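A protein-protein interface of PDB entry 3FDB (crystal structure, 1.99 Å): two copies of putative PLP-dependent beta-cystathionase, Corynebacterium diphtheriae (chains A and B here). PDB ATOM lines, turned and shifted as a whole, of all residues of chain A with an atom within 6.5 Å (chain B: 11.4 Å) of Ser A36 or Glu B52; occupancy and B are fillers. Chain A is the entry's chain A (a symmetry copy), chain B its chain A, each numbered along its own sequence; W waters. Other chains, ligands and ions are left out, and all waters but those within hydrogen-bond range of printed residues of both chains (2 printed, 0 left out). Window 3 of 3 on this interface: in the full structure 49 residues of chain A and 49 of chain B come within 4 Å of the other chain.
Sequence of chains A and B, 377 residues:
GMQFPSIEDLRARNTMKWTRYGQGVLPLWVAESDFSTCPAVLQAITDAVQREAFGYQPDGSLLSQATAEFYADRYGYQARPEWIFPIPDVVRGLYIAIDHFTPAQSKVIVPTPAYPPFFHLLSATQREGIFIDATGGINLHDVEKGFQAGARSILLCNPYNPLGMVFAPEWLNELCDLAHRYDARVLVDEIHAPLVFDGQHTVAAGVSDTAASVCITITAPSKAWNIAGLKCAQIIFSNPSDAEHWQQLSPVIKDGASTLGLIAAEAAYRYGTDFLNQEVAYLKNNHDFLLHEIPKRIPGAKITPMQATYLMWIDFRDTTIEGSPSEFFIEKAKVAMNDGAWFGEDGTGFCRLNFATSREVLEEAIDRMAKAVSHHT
The backbone carbonyl oxygen (O) of Ala A12 is in hydrogen-bond range of the guanidinium group (NH1) of Arg B51, 3.0 Å away.
OE1 of Glu B52 lies within salt-bridge range of NH2 of Arg A13, at 3.0 Å.
The side-chain hydroxyl (OG1) of Thr A37 lies within hydrogen-bond range of the side-chain carboxylate (OE1) of Glu B52.
The side-chain carboxylate (OD2) of Asp B47 is in salt-bridge range of the guanidinium group (NE) of Arg B51, at 2.8 Å.
The backbone NH of Ala B53 is in hydrogen-bond range of the backbone carbonyl oxygen of Ala B48 (3.1 Å).
O of Gly B55 lies within hydrogen-bond range of OG1 of Thr B259 (2.8 Å).
The backbone carbonyl oxygen (O) of Gln A3 lies within hydrogen-bond range of the backbone NH (N) of Ser A36, 2.9 Å away.
The side-chain hydroxyl (OG) of Ser A36 sits close to the backbone NH (N) of Phe A4 (3.3 Å).
The guanidinium group (NH2) of Arg A13 lies within hydrogen-bond range of the backbone carbonyl oxygen (O) of Phe A35, 2.9 Å away.
Among the printed residues, pairs that only touch across the chains: Arg A13 with Arg B51 (3.3 Å), Arg A13 with Ala B53 (3.5 Å), Asn A14 with Arg B51 (3.9 Å), Asn A14 with Pro B58 (3.2 Å), Thr A15 with Gly B55 (3.6 Å), Thr A15 with Tyr B56 (3.3 Å), Thr A15 with Pro B58 (3.9 Å), Ser A36 with Glu B52 (3.9 Å), Thr A37 with Phe B54 (3.6 Å), Leu A42 with Val B49 (3.8 Å), Leu A42 with Glu B52 (3.8 Å), Leu A42 with Phe B54 (3.97 Å) and Asn A226 with Phe B54 (3.5 Å).
Ser A36 touches just one residue of chain B: Glu B52 (3.9 Å).
Glu B52 touches just these residues of chain A: Arg A13, Ser A36, Thr A37 and Leu A42.
No residue of chain B comes within 4 Å of Pro A5.
Phe A35 touches none of the printed residues of chain B.
Cys A38 touches none of the printed residues of chain B.
Of the printed residues of chain B, Leu A42 touches Val B49 (3.8 Å), Glu B52 (3.8 Å) and Phe B54 (3.97 Å).
Printed residues of chain A within 4 Å of Pro B58: Asn A14 and Thr A15.
Of the printed residues of chain A, Phe B54 touches Thr A37 (3.6 Å), Leu A42 (3.97 Å) and Asn A226 (3.5 Å).
Of the printed residues of chain B, Ala A12 touches Arg B51 (3.0 Å).
Thr B46 touches none of the printed residues of chain A.
Asp B47 touches none of the printed residues of chain A.
The nearest residue of chain A that does not touch Glu B52 is Phe A35 (4.6 Å).
The nearest printed residue of chain B that does not touch Asn A14 is Tyr B56 (5.0 Å).
Of the 18 printed residues of chain A, 8 touch a printed residue of chain B.
Printed residues of chain A that touch a printed residue of chain B: Ala A12, Arg A13, Asn A14, Thr A15, Ser A36, Thr A37, Leu A42 and Asn A226.
Hydrophobic or aromatic side chains of chain A that line the printed part of chain B: Leu A42.
Among the printed residues, 16 pairs touch across the chains.
No position is printed for both chains.
Water W2 bridges O of Glu B52 (2.6 Å) and ND2 of Asn A226 (3.4 Å).
Water W1 bridges NH2 of Arg B51 (3.0 Å) and ND2 of Asn A14 (3.1 Å).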
ATOM      1  N   MET A   2       0.323  30.113  22.762  1.00  0.00           N
ATOM      2  CA  MET A   2      -0.648  29.151  23.213  1.00  0.00           C
ATOM      3  C   MET A   2      -0.672  29.213  24.711  1.00  0.00           C
ATOM      4  O   MET A   2       0.324  29.576  25.313  1.00  0.00           O
ATOM      5  CB  MET A   2      -0.184  27.762  22.775  1.00  0.00           C
ATOM      6  CG  MET A   2      -0.191  27.554  21.272  1.00  0.00           C
ATOM      7  SD  MET A   2      -2.006  27.507  20.556  1.00  0.00           S
ATOM      8  CE  MET A   2      -2.355  26.118  21.060  1.00  0.00           C
ATOM      9  N   GLN A   3      -1.796  28.840  25.310  1.00  0.00           N
ATOM     10  CA  GLN A   3      -1.877  28.696  26.749  1.00  0.00           C
ATOM     11  C   GLN A   3      -1.655  27.258  27.114  1.00  0.00           C
ATOM     12  O   GLN A   3      -2.024  26.364  26.347  1.00  0.00           O
ATOM     13  CB  GLN A   3      -3.261  29.085  27.254  1.00  0.00           C
ATOM     14  CG  GLN A   3      -3.591  30.520  27.021  1.00  0.00           C
ATOM     15  CD  GLN A   3      -2.725  31.427  27.845  1.00  0.00           C
ATOM     16  OE1 GLN A   3      -1.899  32.152  27.305  1.00  0.00           O
ATOM     17  NE2 GLN A   3      -2.872  31.356  29.171  1.00  0.00           N
ATOM     18  N   PHE A   4      -1.093  27.036  28.300  1.00  0.00           N
ATOM     19  CA  PHE A   4      -0.926  25.702  28.846  1.00  0.00           C
ATOM     20  C   PHE A   4      -1.446  25.675  30.260  1.00  0.00           C
ATOM     21  O   PHE A   4      -1.275  26.633  30.981  1.00  0.00           O
ATOM     22  CB  PHE A   4       0.554  25.276  28.897  1.00  0.00           C
ATOM     23  CG  PHE A   4       1.188  25.200  27.561  1.00  0.00           C
ATOM     24  CD1 PHE A   4       1.793  26.313  27.009  1.00  0.00           C
ATOM     25  CD2 PHE A   4       1.153  24.012  26.831  1.00  0.00           C
ATOM     26  CE1 PHE A   4       2.335  26.252  25.754  1.00  0.00           C
ATOM     27  CE2 PHE A   4       1.725  23.945  25.574  1.00  0.00           C
ATOM     28  CZ  PHE A   4       2.305  25.088  25.035  1.00  0.00           C
ATOM     29  N   PRO A   5      -2.027  24.559  30.681  1.00  0.00           N
ATOM     30  CA  PRO A   5      -2.343  24.456  32.096  1.00  0.00           C
ATOM     31  C   PRO A   5      -1.050  24.265  32.900  1.00  0.00           C
ATOM     32  O   PRO A   5      -0.004  23.966  32.323  1.00  0.00           O
ATOM     33  CB  PRO A   5      -3.169  23.174  32.190  1.00  0.00           C
ATOM     34  CG  PRO A   5      -3.446  22.727  30.773  1.00  0.00           C
ATOM     35  CD  PRO A   5      -2.375  23.333  29.933  1.00  0.00           C
ATOM     36  N   LEU A  10      -2.300  19.520  34.215  1.00  0.00           N
ATOM     37  CA  LEU A  10      -2.065  18.543  33.118  1.00  0.00           C
ATOM     38  C   LEU A  10      -2.214  17.112  33.638  1.00  0.00           C
ATOM     39  O   LEU A  10      -2.975  16.319  33.094  1.00  0.00           O
ATOM     40  CB  LEU A  10      -0.700  18.778  32.446  1.00  0.00           C
ATOM     41  CG  LEU A  10      -0.649  19.889  31.368  1.00  0.00           C
ATOM     42  CD1 LEU A  10       0.820  20.249  30.932  1.00  0.00           C
ATOM     43  CD2 LEU A  10      -1.512  19.485  30.141  1.00  0.00           C
ATOM     44  N   ALA A  12      -3.792  16.159  36.239  1.00  0.00           N
ATOM     45  CA  ALA A  12      -5.164  16.020  36.698  1.00  0.00           C
ATOM     46  C   ALA A  12      -6.141  15.793  35.560  1.00  0.00           C
ATOM     47  O   ALA A  12      -7.280  15.425  35.835  1.00  0.00           O
ATOM     48  CB  ALA A  12      -5.586  17.224  37.539  1.00  0.00           C
ATOM     49  N   ARG A  13      -5.714  15.992  34.298  1.00  0.00           N
ATOM     50  CA  ARG A  13      -6.524  15.546  33.161  1.00  0.00           C
ATOM     51  C   ARG A  13      -6.787  14.048  33.288  1.00  0.00           C
ATOM     52  O   ARG A  13      -7.828  13.564  32.857  1.00  0.00           O
ATOM     53  CB  ARG A  13      -5.856  15.837  31.821  1.00  0.00           C
ATOM     54  CG  ARG A  13      -5.780  17.290  31.505  1.00  0.00           C
ATOM     55  CD  ARG A  13      -4.992  17.596  30.221  1.00  0.00           C
ATOM     56  NE  ARG A  13      -5.297  18.939  29.756  1.00  0.00           N
ATOM     57  CZ  ARG A  13      -4.937  19.448  28.590  1.00  0.00           C
ATOM     58  NH1 ARG A  13      -4.194  18.747  27.729  1.00  0.00           N
ATOM     59  NH2 ARG A  13      -5.332  20.672  28.277  1.00  0.00           N
ATOM     60  N   ASN A  14      -5.838  13.309  33.878  1.00  0.00           N
ATOM     61  CA  ASN A  14      -6.042  11.882  34.150  1.00  0.00           C
ATOM     62  C   ASN A  14      -6.445  11.087  32.930  1.00  0.00           C
ATOM     63  O   ASN A  14      -7.452  10.362  32.949  1.00  0.00           O
ATOM     64  CB  ASN A  14      -7.078  11.712  35.279  1.00  0.00           C
ATOM     65  CG  ASN A  14      -6.980  10.347  35.970  1.00  0.00           C
ATOM     66  OD1 ASN A  14      -5.891   9.907  36.307  1.00  0.00           O
ATOM     67  ND2 ASN A  14      -8.113   9.689  36.176  1.00  0.00           N
ATOM     68  N   THR A  15      -5.688  11.301  31.838  1.00  0.00           N
ATOM     69  CA  THR A  15      -5.815  10.571  30.584  1.00  0.00           C
ATOM     70  C   THR A  15      -4.653   9.571  30.494  1.00  0.00           C
ATOM     71  O   THR A  15      -3.765   9.546  31.348  1.00  0.00           O
ATOM     72  CB  THR A  15      -5.744  11.517  29.404  1.00  0.00           C
ATOM     73  OG1 THR A  15      -4.471  12.169  29.418  1.00  0.00           O
ATOM     74  CG2 THR A  15      -6.869  12.590  29.503  1.00  0.00           C
ATOM     75  N   ASP A  34      -0.717  19.044  25.039  1.00  0.00           N
ATOM     76  CA  ASP A  34      -0.762  19.653  26.361  1.00  0.00           C
ATOM     77  C   ASP A  34      -1.292  21.094  26.354  1.00  0.00           C
ATOM     78  O   ASP A  34      -1.364  21.747  27.403  1.00  0.00           O
ATOM     79  CB  ASP A  34       0.622  19.594  27.005  1.00  0.00           C
ATOM     80  CG  ASP A  34       1.114  18.165  27.252  1.00  0.00           C
ATOM     81  OD1 ASP A  34       0.340  17.177  27.067  1.00  0.00           O
ATOM     82  OD2 ASP A  34       2.313  18.039  27.621  1.00  0.00           O
ATOM     83  N   PHE A  35      -1.660  21.597  25.177  1.00  0.00           N
ATOM     84  CA  PHE A  35      -2.270  22.921  25.077  1.00  0.00           C
ATOM     85  C   PHE A  35      -3.558  22.956  25.874  1.00  0.00           C
ATOM     86  O   PHE A  35      -4.302  21.968  25.899  1.00  0.00           O
ATOM     87  CB  PHE A  35      -2.611  23.250  23.627  1.00  0.00           C
ATOM     88  CG  PHE A  35      -1.453  23.137  22.690  1.00  0.00           C
ATOM     89  CD1 PHE A  35      -0.321  23.928  22.870  1.00  0.00           C
ATOM     90  CD2 PHE A  35      -1.475  22.232  21.642  1.00  0.00           C
ATOM     91  CE1 PHE A  35       0.762  23.823  22.000  1.00  0.00           C
ATOM     92  CE2 PHE A  35      -0.386  22.136  20.778  1.00  0.00           C
ATOM     93  CZ  PHE A  35       0.729  22.938  20.968  1.00  0.00           C
ATOM     94  N   SER A  36      -3.842  24.098  26.495  1.00  0.00           N
ATOM     95  CA  SER A  36      -5.151  24.308  27.093  1.00  0.00           C
ATOM     96  C   SER A  36      -6.164  24.141  25.962  1.00  0.00           C
ATOM     97  O   SER A  36      -5.966  24.646  24.843  1.00  0.00           O
ATOM     98  CB  SER A  36      -5.249  25.712  27.693  1.00  0.00           C
ATOM     99  OG  SER A  36      -4.199  25.919  28.621  1.00  0.00           O
ATOM    100  N   THR A  37      -7.260  23.447  26.241  1.00  0.00           N
ATOM    101  CA  THR A  37      -8.245  23.160  25.203  1.00  0.00           C
ATOM    102  C   THR A  37      -8.732  24.420  24.501  1.00  0.00           C
ATOM    103  O   THR A  37      -8.985  25.440  25.132  1.00  0.00           O
ATOM    104  CB  THR A  37      -9.453  22.376  25.778  1.00  0.00           C
ATOM    105  OG1 THR A  37      -8.976  21.207  26.447  1.00  0.00           O
ATOM    106  CG2 THR A  37     -10.447  21.977  24.642  1.00  0.00           C
ATOM    107  N   CYS A  38      -8.871  24.357  23.178  1.00  0.00           N
ATOM    108  CA  CYS A  38      -9.442  25.480  22.415  1.00  0.00           C
ATOM    109  C   CYS A  38     -10.682  26.062  23.120  1.00  0.00           C
ATOM    110  O   CYS A  38     -11.634  25.320  23.372  1.00  0.00           O
ATOM    111  CB  CYS A  38      -9.812  24.980  21.013  1.00  0.00           C
ATOM    112  SG  CYS A  38     -10.778  26.135  20.022  1.00  0.00           S
ATOM    113  N   PRO A  39     -10.673  27.375  23.483  1.00  0.00           N
ATOM    114  CA  PRO A  39     -11.821  27.939  24.203  1.00  0.00           C
ATOM    115  C   PRO A  39     -13.192  27.704  23.591  1.00  0.00           C
ATOM    116  O   PRO A  39     -14.162  27.462  24.330  1.00  0.00           O
ATOM    117  CB  PRO A  39     -11.487  29.429  24.280  1.00  0.00           C
ATOM    118  CG  PRO A  39      -9.981  29.429  24.415  1.00  0.00           C
ATOM    119  CD  PRO A  39      -9.567  28.350  23.415  1.00  0.00           C
ATOM    120  N   LEU A  42     -14.022  23.978  24.315  1.00  0.00           N
ATOM    121  CA  LEU A  42     -14.300  23.775  25.726  1.00  0.00           C
ATOM    122  C   LEU A  42     -15.682  24.324  26.103  1.00  0.00           C
ATOM    123  O   LEU A  42     -16.444  23.682  26.840  1.00  0.00           O
ATOM    124  CB  LEU A  42     -13.170  24.397  26.596  1.00  0.00           C
ATOM    125  CG  LEU A  42     -13.289  24.336  28.121  1.00  0.00           C
ATOM    126  CD1 LEU A  42     -13.354  22.862  28.606  1.00  0.00           C
ATOM    127  CD2 LEU A  42     -12.151  25.116  28.753  1.00  0.00           C
ATOM    128  N   ASN A 226      -7.530  18.021  20.159  1.00  0.00           N
ATOM    129  CA  ASN A 226      -7.313  17.231  21.343  1.00  0.00           C
ATOM    130  C   ASN A 226      -8.582  16.782  22.076  1.00  0.00           C
ATOM    131  O   ASN A 226      -8.767  17.041  23.292  1.00  0.00           O
ATOM    132  CB  ASN A 226      -6.343  17.974  22.278  1.00  0.00           C
ATOM    133  CG  ASN A 226      -5.589  17.034  23.202  1.00  0.00           C
ATOM    134  OD1 ASN A 226      -5.050  16.016  22.764  1.00  0.00           O
ATOM    135  ND2 ASN A 226      -5.527  17.379  24.481  1.00  0.00           N
ATOM    136  N   PHE A 275      -7.440  29.302  16.674  1.00  0.00           N
ATOM    137  CA  PHE A 275      -6.654  28.505  17.608  1.00  0.00           C
ATOM    138  C   PHE A 275      -5.718  27.567  16.829  1.00  0.00           C
ATOM    139  O   PHE A 275      -4.536  27.448  17.136  1.00  0.00           O
ATOM    140  CB  PHE A 275      -7.619  27.720  18.506  1.00  0.00           C
ATOM    141  CG  PHE A 275      -6.946  26.703  19.443  1.00  0.00           C
ATOM    142  CD1 PHE A 275      -6.674  25.408  19.012  1.00  0.00           C
ATOM    143  CD2 PHE A 275      -6.654  27.034  20.759  1.00  0.00           C
ATOM    144  CE1 PHE A 275      -6.083  24.473  19.858  1.00  0.00           C
ATOM    145  CE2 PHE A 275      -6.055  26.125  21.599  1.00  0.00           C
ATOM    146  CZ  PHE A 275      -5.790  24.818  21.151  1.00  0.00           C
ATOM    147  N   GLN B  43     -22.381  15.912  38.315  1.00  0.00           N
ATOM    148  CA  GLN B  43     -21.160  16.513  38.879  1.00  0.00           C
ATOM    149  C   GLN B  43     -19.878  15.823  38.407  1.00  0.00           C
ATOM    150  O   GLN B  43     -18.877  16.494  38.170  1.00  0.00           O
ATOM    151  CB  GLN B  43     -21.179  16.574  40.420  1.00  0.00           C
ATOM    152  CG  GLN B  43     -20.013  17.453  41.031  1.00  0.00           C
ATOM    153  CD  GLN B  43     -19.830  18.896  40.372  1.00  0.00           C
ATOM    154  OE1 GLN B  43     -20.796  19.680  40.232  1.00  0.00           O
ATOM    155  NE2 GLN B  43     -18.568  19.229  39.992  1.00  0.00           N
ATOM    156  N   ALA B  44     -19.898  14.494  38.277  1.00  0.00           N
ATOM    157  CA  ALA B  44     -18.728  13.761  37.773  1.00  0.00           C
ATOM    158  C   ALA B  44     -18.384  14.225  36.348  1.00  0.00           C
ATOM    159  O   ALA B  44     -17.206  14.423  36.016  1.00  0.00           O
ATOM    160  CB  ALA B  44     -18.981  12.271  37.792  1.00  0.00           C
ATOM    161  N   ILE B  45     -19.411  14.380  35.512  1.00  0.00           N
ATOM    162  CA  ILE B  45     -19.214  14.823  34.117  1.00  0.00           C
ATOM    163  C   ILE B  45     -18.730  16.283  34.077  1.00  0.00           C
ATOM    164  O   ILE B  45     -17.780  16.635  33.367  1.00  0.00           O
ATOM    165  CB  ILE B  45     -20.511  14.697  33.272  1.00  0.00           C
ATOM    166  CG1 ILE B  45     -20.949  13.227  33.153  1.00  0.00           C
ATOM    167  CG2 ILE B  45     -20.271  15.315  31.876  1.00  0.00           C
ATOM    168  CD1 ILE B  45     -22.411  13.034  32.675  1.00  0.00           C
ATOM    169  N   THR B  46     -19.387  17.122  34.868  1.00  0.00           N
ATOM    170  CA  THR B  46     -19.020  18.526  34.996  1.00  0.00           C
ATOM    171  C   THR B  46     -17.553  18.687  35.435  1.00  0.00           C
ATOM    172  O   THR B  46     -16.822  19.480  34.858  1.00  0.00           O
ATOM    173  CB  THR B  46     -19.964  19.252  35.971  1.00  0.00           C
ATOM    174  OG1 THR B  46     -21.308  19.166  35.482  1.00  0.00           O
ATOM    175  CG2 THR B  46     -19.571  20.715  36.177  1.00  0.00           C
ATOM    176  N   ASP B  47     -17.140  17.962  36.463  1.00  0.00           N
ATOM    177  CA  ASP B  47     -15.768  18.020  36.950  1.00  0.00           C
ATOM    178  C   ASP B  47     -14.754  17.512  35.895  1.00  0.00           C
ATOM    179  O   ASP B  47     -13.669  18.060  35.731  1.00  0.00           O
ATOM    180  CB  ASP B  47     -15.649  17.177  38.214  1.00  0.00           C
ATOM    181  CG  ASP B  47     -14.205  16.953  38.634  1.00  0.00           C
ATOM    182  OD1 ASP B  47     -13.604  17.898  39.188  1.00  0.00           O
ATOM    183  OD2 ASP B  47     -13.668  15.830  38.411  1.00  0.00           O
ATOM    184  N   ALA B  48     -15.108  16.437  35.199  1.00  0.00           N
ATOM    185  CA  ALA B  48     -14.240  15.875  34.167  1.00  0.00           C
ATOM    186  C   ALA B  48     -14.008  16.874  33.026  1.00  0.00           C
ATOM    187  O   ALA B  48     -12.882  16.981  32.509  1.00  0.00           O
ATOM    188  CB  ALA B  48     -14.823  14.538  33.641  1.00  0.00           C
ATOM    189  N   VAL B  49     -15.055  17.615  32.649  1.00  0.00           N
ATOM    190  CA  VAL B  49     -14.943  18.618  31.586  1.00  0.00           C
ATOM    191  C   VAL B  49     -14.038  19.763  32.072  1.00  0.00           C
ATOM    192  O   VAL B  49     -13.163  20.219  31.344  1.00  0.00           O
ATOM    193  CB  VAL B  49     -16.374  19.106  31.103  1.00  0.00           C
ATOM    194  CG1 VAL B  49     -16.280  20.294  30.184  1.00  0.00           C
ATOM    195  CG2 VAL B  49     -17.124  17.957  30.417  1.00  0.00           C
ATOM    196  N   GLN B  50     -14.247  20.220  33.304  1.00  0.00           N
ATOM    197  CA  GLN B  50     -13.413  21.271  33.902  1.00  0.00           C
ATOM    198  C   GLN B  50     -11.948  20.853  33.979  1.00  0.00           C
ATOM    199  O   GLN B  50     -11.046  21.682  33.803  1.00  0.00           O
ATOM    200  CB  GLN B  50     -13.909  21.644  35.310  1.00  0.00           C
ATOM    201  CG  GLN B  50     -15.238  22.421  35.321  1.00  0.00           C
ATOM    202  CD  GLN B  50     -15.890  22.537  36.718  1.00  0.00           C
ATOM    203  OE1 GLN B  50     -15.480  21.867  37.674  1.00  0.00           O
ATOM    204  NE2 GLN B  50     -16.939  23.372  36.819  1.00  0.00           N
ATOM    205  N   ARG B  51     -11.716  19.573  34.212  1.00  0.00           N
ATOM    206  CA  ARG B  51     -10.362  19.005  34.206  1.00  0.00           C
ATOM    207  C   ARG B  51      -9.799  18.733  32.802  1.00  0.00           C
ATOM    208  O   ARG B  51      -8.627  18.378  32.657  1.00  0.00           O
ATOM    209  CB  ARG B  51     -10.340  17.702  35.007  1.00  0.00           C
ATOM    210  CG  ARG B  51     -10.489  17.892  36.518  1.00  0.00           C
ATOM    211  CD  ARG B  51     -10.237  16.585  37.258  1.00  0.00           C
ATOM    212  NE  ARG B  51     -11.266  15.587  36.986  1.00  0.00           N
ATOM    213  CZ  ARG B  51     -11.123  14.507  36.210  1.00  0.00           C
ATOM    214  NH1 ARG B  51      -9.988  14.248  35.550  1.00  0.00           N
ATOM    215  NH2 ARG B  51     -12.151  13.673  36.072  1.00  0.00           N
ATOM    216  N   GLU B  52     -10.632  18.872  31.773  1.00  0.00           N
ATOM    217  CA  GLU B  52     -10.218  18.661  30.389  1.00  0.00           C
ATOM    218  C   GLU B  52      -9.751  17.215  30.155  1.00  0.00           C
ATOM    219  O   GLU B  52      -8.739  16.970  29.508  1.00  0.00           O
ATOM    220  CB  GLU B  52      -9.178  19.698  29.957  1.00  0.00           C
ATOM    221  CG  GLU B  52      -9.715  21.118  30.123  1.00  0.00           C
ATOM    222  CD  GLU B  52      -8.826  22.225  29.604  1.00  0.00           C
ATOM    223  OE1 GLU B  52      -7.954  22.016  28.697  1.00  0.00           O
ATOM    224  OE2 GLU B  52      -9.068  23.350  30.092  1.00  0.00           O
ATOM    225  N   ALA B  53     -10.527  16.271  30.700  1.00  0.00           N
ATOM    226  CA  ALA B  53     -10.325  14.829  30.517  1.00  0.00           C
ATOM    227  C   ALA B  53     -10.828  14.406  29.132  1.00  0.00           C
ATOM    228  O   ALA B  53     -11.830  13.677  29.028  1.00  0.00           O
ATOM    229  CB  ALA B  53     -11.064  14.049  31.613  1.00  0.00           C
ATOM    230  N   PHE B  54     -10.125  14.855  28.081  1.00  0.00           N
ATOM    231  CA  PHE B  54     -10.609  14.663  26.716  1.00  0.00           C
ATOM    232  C   PHE B  54      -9.725  13.776  25.859  1.00  0.00           C
ATOM    233  O   PHE B  54     -10.020  13.556  24.651  1.00  0.00           O
ATOM    234  CB  PHE B  54     -10.745  16.034  26.007  1.00  0.00           C
ATOM    235  CG  PHE B  54     -11.601  17.043  26.741  1.00  0.00           C
ATOM    236  CD1 PHE B  54     -12.744  16.651  27.451  1.00  0.00           C
ATOM    237  CD2 PHE B  54     -11.288  18.394  26.678  1.00  0.00           C
ATOM    238  CE1 PHE B  54     -13.530  17.595  28.096  1.00  0.00           C
ATOM    239  CE2 PHE B  54     -12.066  19.330  27.318  1.00  0.00           C
ATOM    240  CZ  PHE B  54     -13.188  18.931  28.026  1.00  0.00           C
ATOM    241  N   GLY B  55      -8.643  13.274  26.447  1.00  0.00           N
ATOM    242  CA  GLY B  55      -7.710  12.416  25.710  1.00  0.00           C
ATOM    243  C   GLY B  55      -8.133  10.969  25.854  1.00  0.00           C
ATOM    244  O   GLY B  55      -9.302  10.680  26.089  1.00  0.00           O
ATOM    245  N   TYR B  56      -7.172  10.061  25.762  1.00  0.00           N
ATOM    246  CA  TYR B  56      -7.451   8.630  25.843  1.00  0.00           C
ATOM    247  C   TYR B  56      -7.691   8.181  27.273  1.00  0.00           C
ATOM    248  O   TYR B  56      -7.284   8.833  28.234  1.00  0.00           O
ATOM    249  CB  TYR B  56      -6.309   7.823  25.229  1.00  0.00           C
ATOM    250  CG  TYR B  56      -6.145   8.121  23.771  1.00  0.00           C
ATOM    251  CD1 TYR B  56      -7.083   7.674  22.848  1.00  0.00           C
ATOM    252  CD2 TYR B  56      -5.089   8.908  23.316  1.00  0.00           C
ATOM    253  CE1 TYR B  56      -6.947   7.968  21.501  1.00  0.00           C
ATOM    254  CE2 TYR B  56      -4.950   9.209  21.972  1.00  0.00           C
ATOM    255  CZ  TYR B  56      -5.881   8.737  21.077  1.00  0.00           C
ATOM    256  OH  TYR B  56      -5.753   9.054  19.734  1.00  0.00           O
ATOM    257  N   GLN B  57      -8.340   7.043  27.419  1.00  0.00           N
ATOM    258  CA  GLN B  57      -8.712   6.587  28.742  1.00  0.00           C
ATOM    259  C   GLN B  57      -7.517   6.247  29.594  1.00  0.00           C
ATOM    260  O   GLN B  57      -6.537   5.707  29.107  1.00  0.00           O
ATOM    261  CB  GLN B  57      -9.661   5.396  28.660  1.00  0.00           C
ATOM    262  CG  GLN B  57      -9.056   4.092  28.181  1.00  0.00           C
ATOM    263  CD  GLN B  57     -10.166   3.132  27.727  1.00  0.00           C
ATOM    264  OE1 GLN B  57     -10.452   2.142  28.399  1.00  0.00           O
ATOM    265  NE2 GLN B  57     -10.856   3.481  26.625  1.00  0.00           N
ATOM    266  N   PRO B  58      -7.594   6.579  30.888  1.00  0.00           N
ATOM    267  CA  PRO B  58      -6.461   6.314  31.776  1.00  0.00           C
ATOM    268  C   PRO B  58      -6.299   4.877  32.205  1.00  0.00           C
ATOM    269  O   PRO B  58      -7.253   4.079  32.213  1.00  0.00           O
ATOM    270  CB  PRO B  58      -6.779   7.155  33.023  1.00  0.00           C
ATOM    271  CG  PRO B  58      -8.294   7.260  33.048  1.00  0.00           C
ATOM    272  CD  PRO B  58      -8.714   7.254  31.582  1.00  0.00           C
ATOM    273  N   THR B 259     -14.211   8.567  27.020  1.00  0.00           N
ATOM    274  CA  THR B 259     -13.517   8.892  28.253  1.00  0.00           C
ATOM    275  C   THR B 259     -14.476   9.443  29.322  1.00  0.00           C
ATOM    276  O   THR B 259     -14.466   9.001  30.509  1.00  0.00           O
ATOM    277  CB  THR B 259     -12.328   9.856  27.921  1.00  0.00           C
ATOM    278  OG1 THR B 259     -11.396   9.120  27.119  1.00  0.00           O
ATOM    279  CG2 THR B 259     -11.580  10.304  29.157  1.00  0.00           C
ATOM    280  N   LEU B 260     -15.314  10.389  28.901  1.00  0.00           N
ATOM    281  CA  LEU B 260     -16.362  10.943  29.736  1.00  0.00           C
ATOM    282  C   LEU B 260     -17.387   9.898  30.113  1.00  0.00           C
ATOM    283  O   LEU B 260     -17.892   9.893  31.236  1.00  0.00           O
ATOM    284  CB  LEU B 260     -17.045  12.130  29.046  1.00  0.00           C
ATOM    285  CG  LEU B 260     -16.166  13.370  28.906  1.00  0.00           C
ATOM    286  CD1 LEU B 260     -16.935  14.508  28.163  1.00  0.00           C
ATOM    287  CD2 LEU B 260     -15.699  13.846  30.263  1.00  0.00           C
ATOM    288  N   ILE B 263     -16.178   7.768  33.006  1.00  0.00           N
ATOM    289  CA  ILE B 263     -16.295   8.555  34.229  1.00  0.00           C
ATOM    290  C   ILE B 263     -17.764   8.623  34.727  1.00  0.00           C
ATOM    291  O   ILE B 263     -18.023   8.405  35.905  1.00  0.00           O
ATOM    292  CB  ILE B 263     -15.756   9.997  34.021  1.00  0.00           C
ATOM    293  CG1 ILE B 263     -14.220   9.990  33.904  1.00  0.00           C
ATOM    294  CG2 ILE B 263     -16.193  10.879  35.182  1.00  0.00           C
ATOM    295  CD1 ILE B 263     -13.630  11.261  33.244  1.00  0.00           C
HETATM  296  O   HOH W   1     -10.753  11.111  35.331  1.00  0.00           O
HETATM  297  O   HOH W   2      -7.175  16.887  27.407  1.00  0.00           O
